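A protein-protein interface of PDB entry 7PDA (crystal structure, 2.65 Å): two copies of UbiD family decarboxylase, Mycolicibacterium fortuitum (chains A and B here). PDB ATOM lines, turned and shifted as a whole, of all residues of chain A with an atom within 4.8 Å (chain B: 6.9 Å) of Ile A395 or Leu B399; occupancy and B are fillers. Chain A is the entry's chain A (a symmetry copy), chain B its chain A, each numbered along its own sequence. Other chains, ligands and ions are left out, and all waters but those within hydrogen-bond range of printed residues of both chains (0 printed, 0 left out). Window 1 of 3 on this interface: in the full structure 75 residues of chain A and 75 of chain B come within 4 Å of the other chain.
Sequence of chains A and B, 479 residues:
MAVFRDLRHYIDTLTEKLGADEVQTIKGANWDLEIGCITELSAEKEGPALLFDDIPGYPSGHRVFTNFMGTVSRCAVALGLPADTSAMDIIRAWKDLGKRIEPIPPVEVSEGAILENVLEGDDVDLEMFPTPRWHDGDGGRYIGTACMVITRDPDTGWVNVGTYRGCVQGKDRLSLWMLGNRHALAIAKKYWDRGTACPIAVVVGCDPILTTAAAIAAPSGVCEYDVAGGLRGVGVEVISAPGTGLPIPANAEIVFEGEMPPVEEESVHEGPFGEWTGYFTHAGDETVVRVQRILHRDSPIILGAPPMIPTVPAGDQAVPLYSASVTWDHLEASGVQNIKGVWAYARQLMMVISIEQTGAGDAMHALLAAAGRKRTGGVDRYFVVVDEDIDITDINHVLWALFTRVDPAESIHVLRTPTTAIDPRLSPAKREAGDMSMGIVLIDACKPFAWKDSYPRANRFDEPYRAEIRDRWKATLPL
The backbone NH (N) of Asn B396 is in hydrogen-bond range of the side-chain carboxylate (OD1) of Asp B394.
O of Trp B400 sits at hydrogen-bond distance from OG1 of Thr B404, at 3.1 Å.
The side-chain hydroxyl (OH) of Tyr A345 sits at hydrogen-bond distance from the backbone NH (N) of Ile A395, at 3.4 Å.
The side-chain carboxylate of Asp A394 lies within hydrogen-bond range of the backbone NH of Asn A396, at 2.9 Å.
Thr A311 touches Asn B396, and with the chains exchanged Asn A396 touches Thr B311.
Ile A395 touches Leu B399, and with the chains exchanged Leu A399 touches Ile B395.
Positions printed for both chains: 311, 394, 395, 396, 397, 398 and 399.
Ile A395 touches just one residue of chain B: Leu B399.
Leu B399 touches just one residue of chain A: Ile A395.
Printed residues of chain A within 4 Å of Asn B396: Thr A311 (2.7 Å).
Of the printed residues of chain B, Asn A396 touches Thr B311 (2.7 Å).
Printed residues of chain A within 4 Å of Thr B311: Asn A396 (2.7 Å).
Tyr A345 touches none of the printed residues of chain B.
Thr B404 touches none of the printed residues of chain A.
The nearest printed residue of chain B that does not touch Leu A399 is Thr B311 (4.2 Å).
The backbone carbonyl oxygen (O) of Thr B311 sits at hydrogen-bond distance from the side-chain amide nitrogen (ND2) of Asn A396 (2.7 Å).
The side-chain amide nitrogen of Asn B396 is in hydrogen-bond range of the backbone carbonyl oxygen of Thr A311 (2.7 Å).
Among the printed residues, merely in contact across the chains: Leu A399 with Ile B395, Ile A395 with Leu B399, Thr A311 with Trp B400 and Thr A311 with Phe B403.
Hydrophobic or aromatic side chains of chain A that line the printed part of chain B: Ile A395 and Leu A399.
Along chain A the printed residues that touch a printed residue of chain B span positions 311 to 399.
Of the 15 printed residues of chain B, 6 touch a printed residue of chain A.
Hydrophobic or aromatic side chains of chain B that line the printed part of chain A: Ile B395, Leu B399, Trp B400 and Phe B403.
Among the printed residues, 6 pairs touch across the chains.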
ATOM      1  N   THR A 311      26.776 -28.229  16.469  1.00  0.00           N
ATOM      2  CA  THR A 311      27.732 -27.147  16.575  1.00  0.00           C
ATOM      3  C   THR A 311      29.181 -27.627  16.655  1.00  0.00           C
ATOM      4  O   THR A 311      30.093 -26.806  16.694  1.00  0.00           O
ATOM      5  CB  THR A 311      27.479 -26.204  17.758  1.00  0.00           C
ATOM      6  OG1 THR A 311      27.590 -26.929  18.974  1.00  0.00           O
ATOM      7  CG2 THR A 311      26.224 -25.375  17.651  1.00  0.00           C
ATOM      8  N   TYR A 345      25.688 -22.017  10.775  1.00  0.00           N
ATOM      9  CA  TYR A 345      26.122 -22.759  11.955  1.00  0.00           C
ATOM     10  C   TYR A 345      25.054 -23.772  12.377  1.00  0.00           C
ATOM     11  O   TYR A 345      23.869 -23.466  12.354  1.00  0.00           O
ATOM     12  CB  TYR A 345      26.370 -21.780  13.104  1.00  0.00           C
ATOM     13  CG  TYR A 345      27.460 -20.831  12.765  1.00  0.00           C
ATOM     14  CD1 TYR A 345      28.766 -21.241  12.937  1.00  0.00           C
ATOM     15  CD2 TYR A 345      27.198 -19.617  12.121  1.00  0.00           C
ATOM     16  CE1 TYR A 345      29.805 -20.424  12.509  1.00  0.00           C
ATOM     17  CE2 TYR A 345      28.238 -18.764  11.712  1.00  0.00           C
ATOM     18  CZ  TYR A 345      29.549 -19.175  11.932  1.00  0.00           C
ATOM     19  OH  TYR A 345      30.647 -18.467  11.543  1.00  0.00           O
ATOM     20  N   THR A 393      32.442 -16.831   8.500  1.00  0.00           N
ATOM     21  CA  THR A 393      32.838 -18.216   8.713  1.00  0.00           C
ATOM     22  C   THR A 393      33.519 -18.383  10.072  1.00  0.00           C
ATOM     23  O   THR A 393      33.991 -19.477  10.392  1.00  0.00           O
ATOM     24  CB  THR A 393      33.816 -18.711   7.640  1.00  0.00           C
ATOM     25  OG1 THR A 393      35.123 -18.167   7.837  1.00  0.00           O
ATOM     26  CG2 THR A 393      33.330 -18.433   6.240  1.00  0.00           C
ATOM     27  N   ASP A 394      33.615 -17.288  10.829  1.00  0.00           N
ATOM     28  CA  ASP A 394      34.372 -17.237  12.071  1.00  0.00           C
ATOM     29  C   ASP A 394      33.360 -16.810  13.116  1.00  0.00           C
ATOM     30  O   ASP A 394      32.960 -15.635  13.124  1.00  0.00           O
ATOM     31  CB  ASP A 394      35.493 -16.186  12.008  1.00  0.00           C
ATOM     32  CG  ASP A 394      36.207 -15.818  13.313  1.00  0.00           C
ATOM     33  OD1 ASP A 394      35.607 -15.854  14.378  1.00  0.00           O
ATOM     34  OD2 ASP A 394      37.382 -15.460  13.240  1.00  0.00           O
ATOM     35  N   ILE A 395      32.967 -17.783  13.958  1.00  0.00           N
ATOM     36  CA  ILE A 395      31.889 -17.641  14.916  1.00  0.00           C
ATOM     37  C   ILE A 395      32.201 -16.479  15.841  1.00  0.00           C
ATOM     38  O   ILE A 395      31.296 -15.734  16.174  1.00  0.00           O
ATOM     39  CB  ILE A 395      31.653 -18.956  15.694  1.00  0.00           C
ATOM     40  CG1 ILE A 395      30.376 -18.906  16.530  1.00  0.00           C
ATOM     41  CG2 ILE A 395      32.867 -19.294  16.537  1.00  0.00           C
ATOM     42  CD1 ILE A 395      29.197 -18.317  15.806  1.00  0.00           C
ATOM     43  N   ASN A 396      33.464 -16.335  16.239  1.00  0.00           N
ATOM     44  CA  ASN A 396      33.920 -15.259  17.105  1.00  0.00           C
ATOM     45  C   ASN A 396      33.579 -13.916  16.474  1.00  0.00           C
ATOM     46  O   ASN A 396      33.028 -13.037  17.155  1.00  0.00           O
ATOM     47  CB  ASN A 396      35.402 -15.383  17.480  1.00  0.00           C
ATOM     48  CG  ASN A 396      35.674 -16.454  18.538  1.00  0.00           C
ATOM     49  OD1 ASN A 396      34.863 -17.337  18.804  1.00  0.00           O
ATOM     50  ND2 ASN A 396      36.834 -16.393  19.173  1.00  0.00           N
ATOM     51  N   HIS A 397      33.880 -13.775  15.172  1.00  0.00           N
ATOM     52  CA  HIS A 397      33.663 -12.497  14.505  1.00  0.00           C
ATOM     53  C   HIS A 397      32.185 -12.190  14.380  1.00  0.00           C
ATOM     54  O   HIS A 397      31.822 -11.024  14.525  1.00  0.00           O
ATOM     55  CB  HIS A 397      34.274 -12.391  13.110  1.00  0.00           C
ATOM     56  CG  HIS A 397      34.695 -11.002  12.795  1.00  0.00           C
ATOM     57  ND1 HIS A 397      35.055 -10.595  11.504  1.00  0.00           N
ATOM     58  CD2 HIS A 397      34.830  -9.915  13.592  1.00  0.00           C
ATOM     59  CE1 HIS A 397      35.427  -9.329  11.533  1.00  0.00           C
ATOM     60  NE2 HIS A 397      35.275  -8.886  12.805  1.00  0.00           N
ATOM     61  N   VAL A 398      31.371 -13.225  14.091  1.00  0.00           N
ATOM     62  CA  VAL A 398      29.934 -13.060  13.957  1.00  0.00           C
ATOM     63  C   VAL A 398      29.401 -12.679  15.338  1.00  0.00           C
ATOM     64  O   VAL A 398      28.558 -11.792  15.500  1.00  0.00           O
ATOM     65  CB  VAL A 398      29.264 -14.333  13.409  1.00  0.00           C
ATOM     66  CG1 VAL A 398      27.723 -14.302  13.513  1.00  0.00           C
ATOM     67  CG2 VAL A 398      29.725 -14.777  12.018  1.00  0.00           C
ATOM     68  N   LEU A 399      29.936 -13.331  16.367  1.00  0.00           N
ATOM     69  CA  LEU A 399      29.432 -13.025  17.685  1.00  0.00           C
ATOM     70  C   LEU A 399      29.694 -11.551  17.986  1.00  0.00           C
ATOM     71  O   LEU A 399      28.831 -10.853  18.513  1.00  0.00           O
ATOM     72  CB  LEU A 399      30.053 -13.991  18.695  1.00  0.00           C
ATOM     73  CG  LEU A 399      29.344 -15.355  18.844  1.00  0.00           C
ATOM     74  CD1 LEU A 399      30.065 -16.267  19.853  1.00  0.00           C
ATOM     75  CD2 LEU A 399      27.864 -15.228  19.223  1.00  0.00           C
ATOM     76  N   THR B 311      35.924 -10.704  21.445  1.00  0.00           N
ATOM     77  CA  THR B 311      35.627 -12.109  21.267  1.00  0.00           C
ATOM     78  C   THR B 311      36.854 -12.944  20.898  1.00  0.00           C
ATOM     79  O   THR B 311      36.747 -14.161  20.772  1.00  0.00           O
ATOM     80  CB  THR B 311      34.533 -12.391  20.230  1.00  0.00           C
ATOM     81  OG1 THR B 311      34.958 -11.928  18.956  1.00  0.00           O
ATOM     82  CG2 THR B 311      33.153 -11.925  20.621  1.00  0.00           C
ATOM     83  N   MET B 350      27.910 -11.248  26.546  1.00  0.00           N
ATOM     84  CA  MET B 350      26.983 -12.321  26.887  1.00  0.00           C
ATOM     85  C   MET B 350      27.372 -12.864  28.249  1.00  0.00           C
ATOM     86  O   MET B 350      28.483 -13.314  28.404  1.00  0.00           O
ATOM     87  CB  MET B 350      27.098 -13.439  25.859  1.00  0.00           C
ATOM     88  CG  MET B 350      25.920 -14.407  25.832  1.00  0.00           C
ATOM     89  SD  MET B 350      26.135 -15.606  24.444  1.00  0.00           S
ATOM     90  CE  MET B 350      24.994 -14.822  23.309  1.00  0.00           C
ATOM     91  N   ILE B 390      25.332 -28.183  30.304  1.00  0.00           N
ATOM     92  CA  ILE B 390      26.034 -27.366  29.303  1.00  0.00           C
ATOM     93  C   ILE B 390      27.409 -26.917  29.800  1.00  0.00           C
ATOM     94  O   ILE B 390      27.501 -26.282  30.833  1.00  0.00           O
ATOM     95  CB  ILE B 390      25.196 -26.146  28.883  1.00  0.00           C
ATOM     96  CG1 ILE B 390      23.836 -26.585  28.323  1.00  0.00           C
ATOM     97  CG2 ILE B 390      25.994 -25.344  27.882  1.00  0.00           C
ATOM     98  CD1 ILE B 390      23.916 -27.390  27.067  1.00  0.00           C
ATOM     99  N   ASP B 394      32.392 -23.270  26.727  1.00  0.00           N
ATOM    100  CA  ASP B 394      32.590 -23.789  25.382  1.00  0.00           C
ATOM    101  C   ASP B 394      31.471 -23.170  24.567  1.00  0.00           C
ATOM    102  O   ASP B 394      30.310 -23.578  24.728  1.00  0.00           O
ATOM    103  CB  ASP B 394      32.444 -25.320  25.339  1.00  0.00           C
ATOM    104  CG  ASP B 394      32.357 -25.995  23.968  1.00  0.00           C
ATOM    105  OD1 ASP B 394      31.844 -25.412  23.022  1.00  0.00           O
ATOM    106  OD2 ASP B 394      32.789 -27.143  23.867  1.00  0.00           O
ATOM    107  N   ILE B 395      31.855 -22.192  23.726  1.00  0.00           N
ATOM    108  CA  ILE B 395      30.936 -21.352  22.984  1.00  0.00           C
ATOM    109  C   ILE B 395      30.051 -22.234  22.120  1.00  0.00           C
ATOM    110  O   ILE B 395      28.870 -21.953  22.013  1.00  0.00           O
ATOM    111  CB  ILE B 395      31.693 -20.294  22.150  1.00  0.00           C
ATOM    112  CG1 ILE B 395      30.748 -19.252  21.553  1.00  0.00           C
ATOM    113  CG2 ILE B 395      32.535 -20.967  21.084  1.00  0.00           C
ATOM    114  CD1 ILE B 395      29.708 -18.751  22.518  1.00  0.00           C
ATOM    115  N   ASN B 396      30.623 -23.279  21.525  1.00  0.00           N
ATOM    116  CA  ASN B 396      29.901 -24.224  20.687  1.00  0.00           C
ATOM    117  C   ASN B 396      28.754 -24.836  21.479  1.00  0.00           C
ATOM    118  O   ASN B 396      27.619 -24.887  20.980  1.00  0.00           O
ATOM    119  CB  ASN B 396      30.817 -25.279  20.053  1.00  0.00           C
ATOM    120  CG  ASN B 396      31.637 -24.744  18.878  1.00  0.00           C
ATOM    121  OD1 ASN B 396      31.801 -23.543  18.682  1.00  0.00           O
ATOM    122  ND2 ASN B 396      32.171 -25.638  18.060  1.00  0.00           N
ATOM    123  N   HIS B 397      29.047 -25.269  22.716  1.00  0.00           N
ATOM    124  CA  HIS B 397      28.030 -25.941  23.517  1.00  0.00           C
ATOM    125  C   HIS B 397      26.930 -24.981  23.921  1.00  0.00           C
ATOM    126  O   HIS B 397      25.775 -25.401  23.938  1.00  0.00           O
ATOM    127  CB  HIS B 397      28.552 -26.604  24.789  1.00  0.00           C
ATOM    128  CG  HIS B 397      27.768 -27.814  25.144  1.00  0.00           C
ATOM    129  ND1 HIS B 397      27.886 -28.455  26.384  1.00  0.00           N
ATOM    130  CD2 HIS B 397      26.858 -28.521  24.430  1.00  0.00           C
ATOM    131  CE1 HIS B 397      27.110 -29.523  26.398  1.00  0.00           C
ATOM    132  NE2 HIS B 397      26.452 -29.569  25.213  1.00  0.00           N
ATOM    133  N   VAL B 398      27.307 -23.731  24.257  1.00  0.00           N
ATOM    134  CA  VAL B 398      26.344 -22.717  24.649  1.00  0.00           C
ATOM    135  C   VAL B 398      25.489 -22.416  23.419  1.00  0.00           C
ATOM    136  O   VAL B 398      24.263 -22.286  23.480  1.00  0.00           O
ATOM    137  CB  VAL B 398      27.037 -21.455  25.195  1.00  0.00           C
ATOM    138  CG1 VAL B 398      26.075 -20.257  25.361  1.00  0.00           C
ATOM    139  CG2 VAL B 398      27.900 -21.661  26.442  1.00  0.00           C
ATOM    140  N   LEU B 399      26.142 -22.348  22.262  1.00  0.00           N
ATOM    141  CA  LEU B 399      25.374 -22.029  21.081  1.00  0.00           C
ATOM    142  C   LEU B 399      24.323 -23.115  20.864  1.00  0.00           C
ATOM    143  O   LEU B 399      23.170 -22.823  20.555  1.00  0.00           O
ATOM    144  CB  LEU B 399      26.329 -21.837  19.901  1.00  0.00           C
ATOM    145  CG  LEU B 399      26.950 -20.430  19.760  1.00  0.00           C
ATOM    146  CD1 LEU B 399      27.921 -20.350  18.569  1.00  0.00           C
ATOM    147  CD2 LEU B 399      25.902 -19.315  19.655  1.00  0.00           C
ATOM    148  N   TRP B 400      24.692 -24.381  21.096  1.00  0.00           N
ATOM    149  CA  TRP B 400      23.771 -25.412  20.677  1.00  0.00           C
ATOM    150  C   TRP B 400      22.567 -25.314  21.595  1.00  0.00           C
ATOM    151  O   TRP B 400      21.429 -25.547  21.174  1.00  0.00           O
ATOM    152  CB  TRP B 400      24.455 -26.779  20.655  1.00  0.00           C
ATOM    153  CG  TRP B 400      23.577 -27.983  20.706  1.00  0.00           C
ATOM    154  CD1 TRP B 400      22.948 -28.598  19.660  1.00  0.00           C
ATOM    155  CD2 TRP B 400      23.276 -28.769  21.870  1.00  0.00           C
ATOM    156  NE1 TRP B 400      22.309 -29.742  20.086  1.00  0.00           N
ATOM    157  CE2 TRP B 400      22.468 -29.857  21.449  1.00  0.00           C
ATOM    158  CE3 TRP B 400      23.623 -28.684  23.221  1.00  0.00           C
ATOM    159  CZ2 TRP B 400      21.992 -30.831  22.340  1.00  0.00           C
ATOM    160  CZ3 TRP B 400      23.153 -29.653  24.095  1.00  0.00           C
ATOM    161  CH2 TRP B 400      22.351 -30.725  23.666  1.00  0.00           C
ATOM    162  N   ALA B 401      22.829 -24.859  22.816  1.00  0.00           N
ATOM    163  CA  ALA B 401      21.715 -24.700  23.726  1.00  0.00           C
ATOM    164  C   ALA B 401      20.890 -23.533  23.247  1.00  0.00           C
ATOM    165  O   ALA B 401      19.664 -23.682  23.257  1.00  0.00           O
ATOM    166  CB  ALA B 401      22.089 -24.618  25.197  1.00  0.00           C
ATOM    167  N   LEU B 402      21.537 -22.413  22.826  1.00  0.00           N
ATOM    168  CA  LEU B 402      20.686 -21.315  22.359  1.00  0.00           C
ATOM    169  C   LEU B 402      19.942 -21.759  21.098  1.00  0.00           C
ATOM    170  O   LEU B 402      18.867 -21.261  20.772  1.00  0.00           O
ATOM    171  CB  LEU B 402      21.443 -20.022  22.038  1.00  0.00           C
ATOM    172  CG  LEU B 402      22.052 -19.226  23.186  1.00  0.00           C
ATOM    173  CD1 LEU B 402      23.256 -18.393  22.666  1.00  0.00           C
ATOM    174  CD2 LEU B 402      20.982 -18.369  23.845  1.00  0.00           C
ATOM    175  N   PHE B 403      20.562 -22.643  20.330  1.00  0.00           N
ATOM    176  CA  PHE B 403      19.954 -23.086  19.086  1.00  0.00           C
ATOM    177  C   PHE B 403      18.888 -24.159  19.325  1.00  0.00           C
ATOM    178  O   PHE B 403      18.022 -24.315  18.477  1.00  0.00           O
ATOM    179  CB  PHE B 403      21.012 -23.708  18.181  1.00  0.00           C
ATOM    180  CG  PHE B 403      21.988 -22.722  17.622  1.00  0.00           C
ATOM    181  CD1 PHE B 403      21.794 -21.346  17.838  1.00  0.00           C
ATOM    182  CD2 PHE B 403      23.072 -23.156  16.876  1.00  0.00           C
ATOM    183  CE1 PHE B 403      22.678 -20.405  17.355  1.00  0.00           C
ATOM    184  CE2 PHE B 403      23.944 -22.199  16.361  1.00  0.00           C
ATOM    185  CZ  PHE B 403      23.757 -20.835  16.607  1.00  0.00           C
ATOM    186  N   THR B 404      18.963 -24.959  20.411  1.00  0.00           N
ATOM    187  CA  THR B 404      18.014 -26.089  20.471  1.00  0.00           C
ATOM    188  C   THR B 404      17.197 -26.148  21.757  1.00  0.00           C
ATOM    189  O   THR B 404      16.391 -27.044  21.889  1.00  0.00           O
ATOM    190  CB  THR B 404      18.626 -27.480  20.277  1.00  0.00           C
ATOM    191  OG1 THR B 404      19.267 -27.702  21.525  1.00  0.00           O
ATOM    192  CG2 THR B 404      19.600 -27.605  19.129  1.00  0.00           C
ATOM    193  N   ARG B 405      17.371 -25.194  22.682  1.00  0.00           N
ATOM    194  CA  ARG B 405      16.581 -25.214  23.905  1.00  0.00           C
ATOM    195  C   ARG B 405      15.793 -23.916  24.135  1.00  0.00           C
ATOM    196  O   ARG B 405      15.330 -23.668  25.236  1.00  0.00           O
ATOM    197  CB  ARG B 405      17.382 -25.713  25.123  1.00  0.00           C
ATOM    198  CG  ARG B 405      18.157 -26.999  24.903  1.00  0.00           C
ATOM    199  CD  ARG B 405      19.047 -27.282  26.119  1.00  0.00           C
ATOM    200  NE  ARG B 405      19.616 -28.654  26.087  1.00  0.00           N
ATOM    201  CZ  ARG B 405      20.266 -29.228  27.097  1.00  0.00           C
ATOM    202  NH1 ARG B 405      20.446 -28.551  28.214  1.00  0.00           N
ATOM    203  NH2 ARG B 405      20.773 -30.439  26.992  1.00  0.00           N
